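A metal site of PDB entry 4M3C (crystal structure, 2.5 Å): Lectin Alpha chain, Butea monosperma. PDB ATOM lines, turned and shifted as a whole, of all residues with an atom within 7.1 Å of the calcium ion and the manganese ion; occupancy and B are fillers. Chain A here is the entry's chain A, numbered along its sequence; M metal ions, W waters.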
ATOM      1  N   ASP A  88      -0.311  10.572 -15.158  1.00  0.00           N
ATOM      2  CA  ASP A  88      -0.617   9.750 -16.336  1.00  0.00           C
ATOM      3  C   ASP A  88      -2.101   9.803 -16.760  1.00  0.00           C
ATOM      4  O   ASP A  88      -2.445   9.394 -17.873  1.00  0.00           O
ATOM      5  CB  ASP A  88      -0.257   8.287 -16.100  1.00  0.00           C
ATOM      6  CG  ASP A  88       1.146   7.934 -16.544  1.00  0.00           C
ATOM      7  OD1 ASP A  88       1.969   7.755 -15.634  1.00  0.00           O
ATOM      8  OD2 ASP A  88       1.444   7.803 -17.757  1.00  0.00           O
ATOM      9  N   GLY A  89      -2.961  10.279 -15.861  1.00  0.00           N
ATOM     10  CA  GLY A  89      -4.404  10.367 -16.178  1.00  0.00           C
ATOM     11  C   GLY A  89      -5.316   9.755 -15.116  1.00  0.00           C
ATOM     12  O   GLY A  89      -4.843   9.203 -14.115  1.00  0.00           O
ATOM     13  N   ALA A 105       1.222   4.300 -12.991  1.00  0.00           N
ATOM     14  CA  ALA A 105       1.655   4.969 -14.224  1.00  0.00           C
ATOM     15  C   ALA A 105       0.581   4.750 -15.343  1.00  0.00           C
ATOM     16  O   ALA A 105      -0.613   4.816 -15.065  1.00  0.00           O
ATOM     17  CB  ALA A 105       3.036   4.473 -14.641  1.00  0.00           C
ATOM     18  N   GLY A 106       1.013   4.477 -16.575  1.00  0.00           N
ATOM     19  CA  GLY A 106       0.091   4.396 -17.717  1.00  0.00           C
ATOM     20  C   GLY A 106      -0.935   3.264 -17.696  1.00  0.00           C
ATOM     21  O   GLY A 106      -1.850   3.252 -18.523  1.00  0.00           O
ATOM     22  N   PHE A 107      -0.790   2.326 -16.770  1.00  0.00           N
ATOM     23  CA  PHE A 107      -1.841   1.326 -16.521  1.00  0.00           C
ATOM     24  C   PHE A 107      -3.002   1.901 -15.716  1.00  0.00           C
ATOM     25  O   PHE A 107      -4.058   1.263 -15.587  1.00  0.00           O
ATOM     26  CB  PHE A 107      -1.289   0.119 -15.779  1.00  0.00           C
ATOM     27  CG  PHE A 107      -0.013  -0.443 -16.356  1.00  0.00           C
ATOM     28  CD1 PHE A 107      -0.055  -1.458 -17.318  1.00  0.00           C
ATOM     29  CD2 PHE A 107       1.207   0.007 -15.910  1.00  0.00           C
ATOM     30  CE1 PHE A 107       1.123  -2.003 -17.828  1.00  0.00           C
ATOM     31  CE2 PHE A 107       2.373  -0.535 -16.401  1.00  0.00           C
ATOM     32  CZ  PHE A 107       2.334  -1.543 -17.357  1.00  0.00           C
ATOM     33  N   LEU A 108      -2.806   3.088 -15.164  1.00  0.00           N
ATOM     34  CA  LEU A 108      -3.880   3.859 -14.570  1.00  0.00           C
ATOM     35  C   LEU A 108      -4.626   3.145 -13.441  1.00  0.00           C
ATOM     36  O   LEU A 108      -5.694   3.604 -13.016  1.00  0.00           O
ATOM     37  CB  LEU A 108      -4.878   4.293 -15.662  1.00  0.00           C
ATOM     38  CG  LEU A 108      -4.400   5.304 -16.718  1.00  0.00           C
ATOM     39  CD1 LEU A 108      -5.550   5.637 -17.665  1.00  0.00           C
ATOM     40  CD2 LEU A 108      -3.827   6.572 -16.084  1.00  0.00           C
ATOM     41  N   GLU A 126     -11.172   6.296 -19.807  1.00  0.00           N
ATOM     42  CA  GLU A 126      -9.939   6.944 -19.390  1.00  0.00           C
ATOM     43  C   GLU A 126      -9.790   8.354 -19.934  1.00  0.00           C
ATOM     44  O   GLU A 126     -10.204   8.673 -21.059  1.00  0.00           O
ATOM     45  CB  GLU A 126      -8.707   6.117 -19.752  1.00  0.00           C
ATOM     46  CG  GLU A 126      -8.549   5.851 -21.241  1.00  0.00           C
ATOM     47  CD  GLU A 126      -7.152   5.352 -21.643  1.00  0.00           C
ATOM     48  OE1 GLU A 126      -6.714   4.283 -21.157  1.00  0.00           O
ATOM     49  OE2 GLU A 126      -6.485   6.049 -22.445  1.00  0.00           O
ATOM     50  N   PHE A 127      -9.177   9.183 -19.094  1.00  0.00           N
ATOM     51  CA  PHE A 127      -8.862  10.519 -19.437  1.00  0.00           C
ATOM     52  C   PHE A 127      -7.351  10.548 -19.337  1.00  0.00           C
ATOM     53  O   PHE A 127      -6.799  10.743 -18.282  1.00  0.00           O
ATOM     54  CB  PHE A 127      -9.567  11.444 -18.444  1.00  0.00           C
ATOM     55  CG  PHE A 127     -11.058  11.377 -18.553  1.00  0.00           C
ATOM     56  CD1 PHE A 127     -11.740  12.197 -19.413  1.00  0.00           C
ATOM     57  CD2 PHE A 127     -11.783  10.430 -17.824  1.00  0.00           C
ATOM     58  CE1 PHE A 127     -13.105  12.098 -19.564  1.00  0.00           C
ATOM     59  CE2 PHE A 127     -13.170  10.344 -17.932  1.00  0.00           C
ATOM     60  CZ  PHE A 127     -13.836  11.178 -18.816  1.00  0.00           C
ATOM     61  N   ASP A 128      -6.711  10.310 -20.478  1.00  0.00           N
ATOM     62  CA  ASP A 128      -5.329   9.830 -20.576  1.00  0.00           C
ATOM     63  C   ASP A 128      -4.380  10.911 -21.061  1.00  0.00           C
ATOM     64  O   ASP A 128      -4.574  11.531 -22.128  1.00  0.00           O
ATOM     65  CB  ASP A 128      -5.268   8.653 -21.537  1.00  0.00           C
ATOM     66  CG  ASP A 128      -3.884   8.027 -21.663  1.00  0.00           C
ATOM     67  OD1 ASP A 128      -3.817   6.949 -22.296  1.00  0.00           O
ATOM     68  OD2 ASP A 128      -2.886   8.636 -21.183  1.00  0.00           O
ATOM     69  N   THR A 129      -3.301  11.066 -20.304  1.00  0.00           N
ATOM     70  CA  THR A 129      -2.659  12.376 -20.198  1.00  0.00           C
ATOM     71  C   THR A 129      -1.207  12.377 -20.721  1.00  0.00           C
ATOM     72  O   THR A 129      -0.630  13.426 -21.013  1.00  0.00           O
ATOM     73  CB  THR A 129      -2.871  12.882 -18.765  1.00  0.00           C
ATOM     74  OG1 THR A 129      -3.566  14.136 -18.778  1.00  0.00           O
ATOM     75  CG2 THR A 129      -1.651  12.920 -17.945  1.00  0.00           C
ATOM     76  N   TYR A 130      -0.682  11.172 -20.910  1.00  0.00           N
ATOM     77  CA  TYR A 130       0.680  10.894 -21.353  1.00  0.00           C
ATOM     78  C   TYR A 130       0.667   9.760 -22.409  1.00  0.00           C
ATOM     79  O   TYR A 130       0.078   8.689 -22.186  1.00  0.00           O
ATOM     80  CB  TYR A 130       1.482  10.444 -20.143  1.00  0.00           C
ATOM     81  CG  TYR A 130       2.884   9.972 -20.481  1.00  0.00           C
ATOM     82  CD1 TYR A 130       3.911  10.893 -20.649  1.00  0.00           C
ATOM     83  CD2 TYR A 130       3.158   8.623 -20.668  1.00  0.00           C
ATOM     84  CE1 TYR A 130       5.178  10.497 -20.981  1.00  0.00           C
ATOM     85  CE2 TYR A 130       4.435   8.200 -20.985  1.00  0.00           C
ATOM     86  CZ  TYR A 130       5.446   9.137 -21.133  1.00  0.00           C
ATOM     87  OH  TYR A 130       6.755   8.761 -21.458  1.00  0.00           O
ATOM     88  N   GLU A 131       1.318   9.993 -23.546  1.00  0.00           N
ATOM     89  CA  GLU A 131       1.327   9.001 -24.628  1.00  0.00           C
ATOM     90  C   GLU A 131       2.286   7.867 -24.318  1.00  0.00           C
ATOM     91  O   GLU A 131       3.481   8.066 -24.129  1.00  0.00           O
ATOM     92  CB  GLU A 131       1.645   9.614 -25.996  1.00  0.00           C
ATOM     93  CG  GLU A 131       1.784   8.559 -27.099  1.00  0.00           C
ATOM     94  CD  GLU A 131       2.182   9.137 -28.454  1.00  0.00           C
ATOM     95  OE1 GLU A 131       3.141   9.942 -28.543  1.00  0.00           O
ATOM     96  OE2 GLU A 131       1.518   8.799 -29.445  1.00  0.00           O
ATOM     97  N   ASN A 132       1.728   6.661 -24.272  1.00  0.00           N
ATOM     98  CA  ASN A 132       2.475   5.440 -24.188  1.00  0.00           C
ATOM     99  C   ASN A 132       2.333   4.746 -25.535  1.00  0.00           C
ATOM    100  O   ASN A 132       1.274   4.156 -25.810  1.00  0.00           O
ATOM    101  CB  ASN A 132       1.895   4.564 -23.082  1.00  0.00           C
ATOM    102  CG  ASN A 132       1.709   5.308 -21.770  1.00  0.00           C
ATOM    103  OD1 ASN A 132       2.629   5.381 -20.960  1.00  0.00           O
ATOM    104  ND2 ASN A 132       0.508   5.858 -21.549  1.00  0.00           N
ATOM    105  N   PHE A 135       1.169   1.235 -25.622  1.00  0.00           N
ATOM    106  CA  PHE A 135      -0.278   0.958 -25.487  1.00  0.00           C
ATOM    107  C   PHE A 135      -1.068   1.455 -26.679  1.00  0.00           C
ATOM    108  O   PHE A 135      -2.301   1.633 -26.584  1.00  0.00           O
ATOM    109  CB  PHE A 135      -0.819   1.687 -24.251  1.00  0.00           C
ATOM    110  CG  PHE A 135      -0.181   1.278 -22.960  1.00  0.00           C
ATOM    111  CD1 PHE A 135       0.473   0.039 -22.832  1.00  0.00           C
ATOM    112  CD2 PHE A 135      -0.273   2.108 -21.834  1.00  0.00           C
ATOM    113  CE1 PHE A 135       1.057  -0.336 -21.633  1.00  0.00           C
ATOM    114  CE2 PHE A 135       0.314   1.740 -20.629  1.00  0.00           C
ATOM    115  CZ  PHE A 135       0.975   0.513 -20.519  1.00  0.00           C
ATOM    116  N   LEU A 136      -0.361   1.754 -27.772  1.00  0.00           N
ATOM    117  CA  LEU A 136      -0.963   2.367 -28.955  1.00  0.00           C
ATOM    118  C   LEU A 136      -1.720   3.686 -28.652  1.00  0.00           C
ATOM    119  O   LEU A 136      -2.685   4.006 -29.350  1.00  0.00           O
ATOM    120  CB  LEU A 136      -1.843   1.346 -29.706  1.00  0.00           C
ATOM    121  CG  LEU A 136      -1.430  -0.134 -29.947  1.00  0.00           C
ATOM    122  CD1 LEU A 136      -2.353  -0.794 -30.970  1.00  0.00           C
ATOM    123  CD2 LEU A 136       0.031  -0.262 -30.388  1.00  0.00           C
ATOM    124  N   ASP A 137      -1.280   4.434 -27.635  1.00  0.00           N
ATOM    125  CA  ASP A 137      -1.834   5.757 -27.351  1.00  0.00           C
ATOM    126  C   ASP A 137      -1.695   6.697 -28.567  1.00  0.00           C
ATOM    127  O   ASP A 137      -0.691   6.668 -29.261  1.00  0.00           O
ATOM    128  CB  ASP A 137      -1.126   6.413 -26.149  1.00  0.00           C
ATOM    129  CG  ASP A 137      -1.700   5.997 -24.801  1.00  0.00           C
ATOM    130  OD1 ASP A 137      -2.754   5.344 -24.754  1.00  0.00           O
ATOM    131  OD2 ASP A 137      -1.102   6.341 -23.757  1.00  0.00           O
ATOM    132  N   PRO A 138      -2.726   7.525 -28.834  1.00  0.00           N
ATOM    133  CA  PRO A 138      -2.617   8.611 -29.822  1.00  0.00           C
ATOM    134  C   PRO A 138      -1.664   9.686 -29.309  1.00  0.00           C
ATOM    135  O   PRO A 138      -1.416   9.726 -28.113  1.00  0.00           O
ATOM    136  CB  PRO A 138      -4.050   9.175 -29.884  1.00  0.00           C
ATOM    137  CG  PRO A 138      -4.670   8.770 -28.583  1.00  0.00           C
ATOM    138  CD  PRO A 138      -4.096   7.422 -28.277  1.00  0.00           C
ATOM    139  N   HIS A 142      -6.301  12.436 -24.744  1.00  0.00           N
ATOM    140  CA  HIS A 142      -7.442  11.761 -25.334  1.00  0.00           C
ATOM    141  C   HIS A 142      -8.327  11.102 -24.323  1.00  0.00           C
ATOM    142  O   HIS A 142      -7.841  10.605 -23.315  1.00  0.00           O
ATOM    143  CB  HIS A 142      -6.970  10.705 -26.314  1.00  0.00           C
ATOM    144  CG  HIS A 142      -5.947   9.757 -25.731  1.00  0.00           C
ATOM    145  ND1 HIS A 142      -4.716  10.155 -25.357  1.00  0.00           N
ATOM    146  CD2 HIS A 142      -6.020   8.388 -25.442  1.00  0.00           C
ATOM    147  CE1 HIS A 142      -4.032   9.101 -24.855  1.00  0.00           C
ATOM    148  NE2 HIS A 142      -4.828   8.023 -24.913  1.00  0.00           N
ATOM    149  N   ILE A 143      -9.629  11.100 -24.628  1.00  0.00           N
ATOM    150  CA  ILE A 143     -10.585  10.269 -23.924  1.00  0.00           C
ATOM    151  C   ILE A 143     -10.553   8.897 -24.547  1.00  0.00           C
ATOM    152  O   ILE A 143     -10.498   8.759 -25.771  1.00  0.00           O
ATOM    153  CB  ILE A 143     -11.998  10.812 -24.036  1.00  0.00           C
ATOM    154  CG1 ILE A 143     -12.083  12.178 -23.350  1.00  0.00           C
ATOM    155  CG2 ILE A 143     -12.981   9.808 -23.417  1.00  0.00           C
ATOM    156  CD1 ILE A 143     -13.298  12.987 -23.739  1.00  0.00           C
ATOM    157  N   GLY A 144     -10.591   7.872 -23.704  1.00  0.00           N
ATOM    158  CA  GLY A 144     -10.383   6.509 -24.204  1.00  0.00           C
ATOM    159  C   GLY A 144     -11.378   5.513 -23.641  1.00  0.00           C
ATOM    160  O   GLY A 144     -11.806   5.615 -22.492  1.00  0.00           O
ATOM    161  N   ASP A 146     -11.497   1.769 -22.547  1.00  0.00           N
ATOM    162  CA  ASP A 146     -10.733   0.537 -22.216  1.00  0.00           C
ATOM    163  C   ASP A 146     -11.584  -0.675 -21.768  1.00  0.00           C
ATOM    164  O   ASP A 146     -12.276  -0.654 -20.729  1.00  0.00           O
ATOM    165  CB  ASP A 146      -9.719   0.798 -21.129  1.00  0.00           C
ATOM    166  CG  ASP A 146      -8.968   2.079 -21.302  1.00  0.00           C
ATOM    167  OD1 ASP A 146      -8.508   2.580 -20.256  1.00  0.00           O
ATOM    168  OD2 ASP A 146      -8.799   2.571 -22.451  1.00  0.00           O
ATOM    169  N   ILE A 150      -6.263  -1.613 -21.493  1.00  0.00           N
ATOM    170  CA  ILE A 150      -5.415  -0.365 -21.509  1.00  0.00           C
ATOM    171  C   ILE A 150      -5.088   0.229 -22.890  1.00  0.00           C
ATOM    172  O   ILE A 150      -4.818   1.425 -23.013  1.00  0.00           O
ATOM    173  CB  ILE A 150      -4.106  -0.414 -20.626  1.00  0.00           C
ATOM    174  CG1 ILE A 150      -3.556   0.998 -20.362  1.00  0.00           C
ATOM    175  CG2 ILE A 150      -2.978  -1.155 -21.317  1.00  0.00           C
ATOM    176  CD1 ILE A 150      -4.521   1.995 -19.770  1.00  0.00           C
ATOM    177  N   LYS A 151      -5.082  -0.650 -23.898  1.00  0.00           N
ATOM    178  CA  LYS A 151      -5.048  -0.279 -25.293  1.00  0.00           C
ATOM    179  C   LYS A 151      -6.490   0.037 -25.672  1.00  0.00           C
ATOM    180  O   LYS A 151      -7.220  -0.848 -25.997  1.00  0.00           O
ATOM    181  CB  LYS A 151      -4.576  -1.453 -26.167  1.00  0.00           C
ATOM    182  CG  LYS A 151      -3.082  -1.768 -26.119  1.00  0.00           C
ATOM    183  CD  LYS A 151      -2.790  -3.015 -26.960  1.00  0.00           C
ATOM    184  CE  LYS A 151      -1.325  -3.469 -26.955  1.00  0.00           C
ATOM    185  NZ  LYS A 151      -1.139  -4.697 -27.797  1.00  0.00           N
ATOM    186  N   SER A 152      -6.880   1.302 -25.650  1.00  0.00           N
ATOM    187  CA  SER A 152      -8.264   1.668 -25.864  1.00  0.00           C
ATOM    188  C   SER A 152      -8.817   1.049 -27.126  1.00  0.00           C
ATOM    189  O   SER A 152      -8.150   1.071 -28.144  1.00  0.00           O
ATOM    190  CB  SER A 152      -8.376   3.181 -25.943  1.00  0.00           C
ATOM    191  OG  SER A 152      -7.622   3.766 -24.905  1.00  0.00           O
ATOM    192  N   THR A 155     -10.533   5.894 -29.292  1.00  0.00           N
ATOM    193  CA  THR A 155     -10.134   7.150 -28.624  1.00  0.00           C
ATOM    194  C   THR A 155     -10.605   8.394 -29.431  1.00  0.00           C
ATOM    195  O   THR A 155     -10.999   8.270 -30.592  1.00  0.00           O
ATOM    196  CB  THR A 155      -8.598   7.227 -28.461  1.00  0.00           C
ATOM    197  OG1 THR A 155      -7.970   7.174 -29.757  1.00  0.00           O
ATOM    198  CG2 THR A 155      -8.065   6.069 -27.657  1.00  0.00           C
HETATM  199 CA    CA M   1      -1.307   6.929 -21.427  1.00  0.00          CA
HETATM  200 MN    MN M   2      -4.724   5.858 -23.899  1.00  0.00          MN
HETATM  201  O   HOH W   1      -1.933   4.938 -20.705  1.00  0.00           O
HETATM  202  O   HOH W   2      -4.263   4.362 -22.584  1.00  0.00           O
HETATM  203  O   HOH W   3      -4.865   3.655 -26.068  1.00  0.00           O
HETATM  204  O   HOH W   4      -0.847   7.536 -19.308  1.00  0.00           O
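OE1 of Glu 126 lies close to OD1 of Asp 146, 2.6 Å away.
The backbone carbonyl oxygen (O) of Glu 126 lies within hydrogen-bond range of the backbone NH (N) of Gly 144, at 2.8 Å.
The side-chain carboxylate (OD2) of Asp 146 lies within hydrogen-bond range of the side-chain hydroxyl (OG) of Ser 152 (3.0 Å).
Water W2 lies within hydrogen-bond range of the side-chain carboxylate of Glu 126 (2.8 Å) and the backbone carbonyl oxygen of Ile 150 (3.0 Å).
Water W3 bridges the side-chain hydroxyl of Ser 152 and the backbone carbonyl oxygen of Phe 135.
The manganese ion is bound by water W2 (2.0 Å).
OD1 of Asp 128 is bound to the manganese ion, at 2.1 Å.
OD1 of Asp 137 is bound to the manganese ion, 2.2 Å away.
OE2 of Glu 126 is bound to the manganese ion, at 2.3 Å.
The manganese ion is bound by NE2 of His 142, at 2.4 Å.
Within 4 Å of the calcium ion: Asp 128, Tyr 130, Asn 132 and Asp 137.
The nearest printed residue that does not touch the calcium ion is Asp 88 (4.5 Å).
The calcium ion is bound by ND2 of Asn 132 (2.1 Å), water W1 (2.2 Å), water W4 (2.3 Å), OD2 of Asp 128 (2.3 Å), O of Tyr 130 (2.4 Å), OD2 of Asp 137 (2.4 Å) and OD1 of Asp 128 (2.7 Å).
Ser 152 touches the manganese ion (OG to MN, 3.7 Å).
Of the 25 residues printed, 5 come within 4 Å of the manganese ion.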
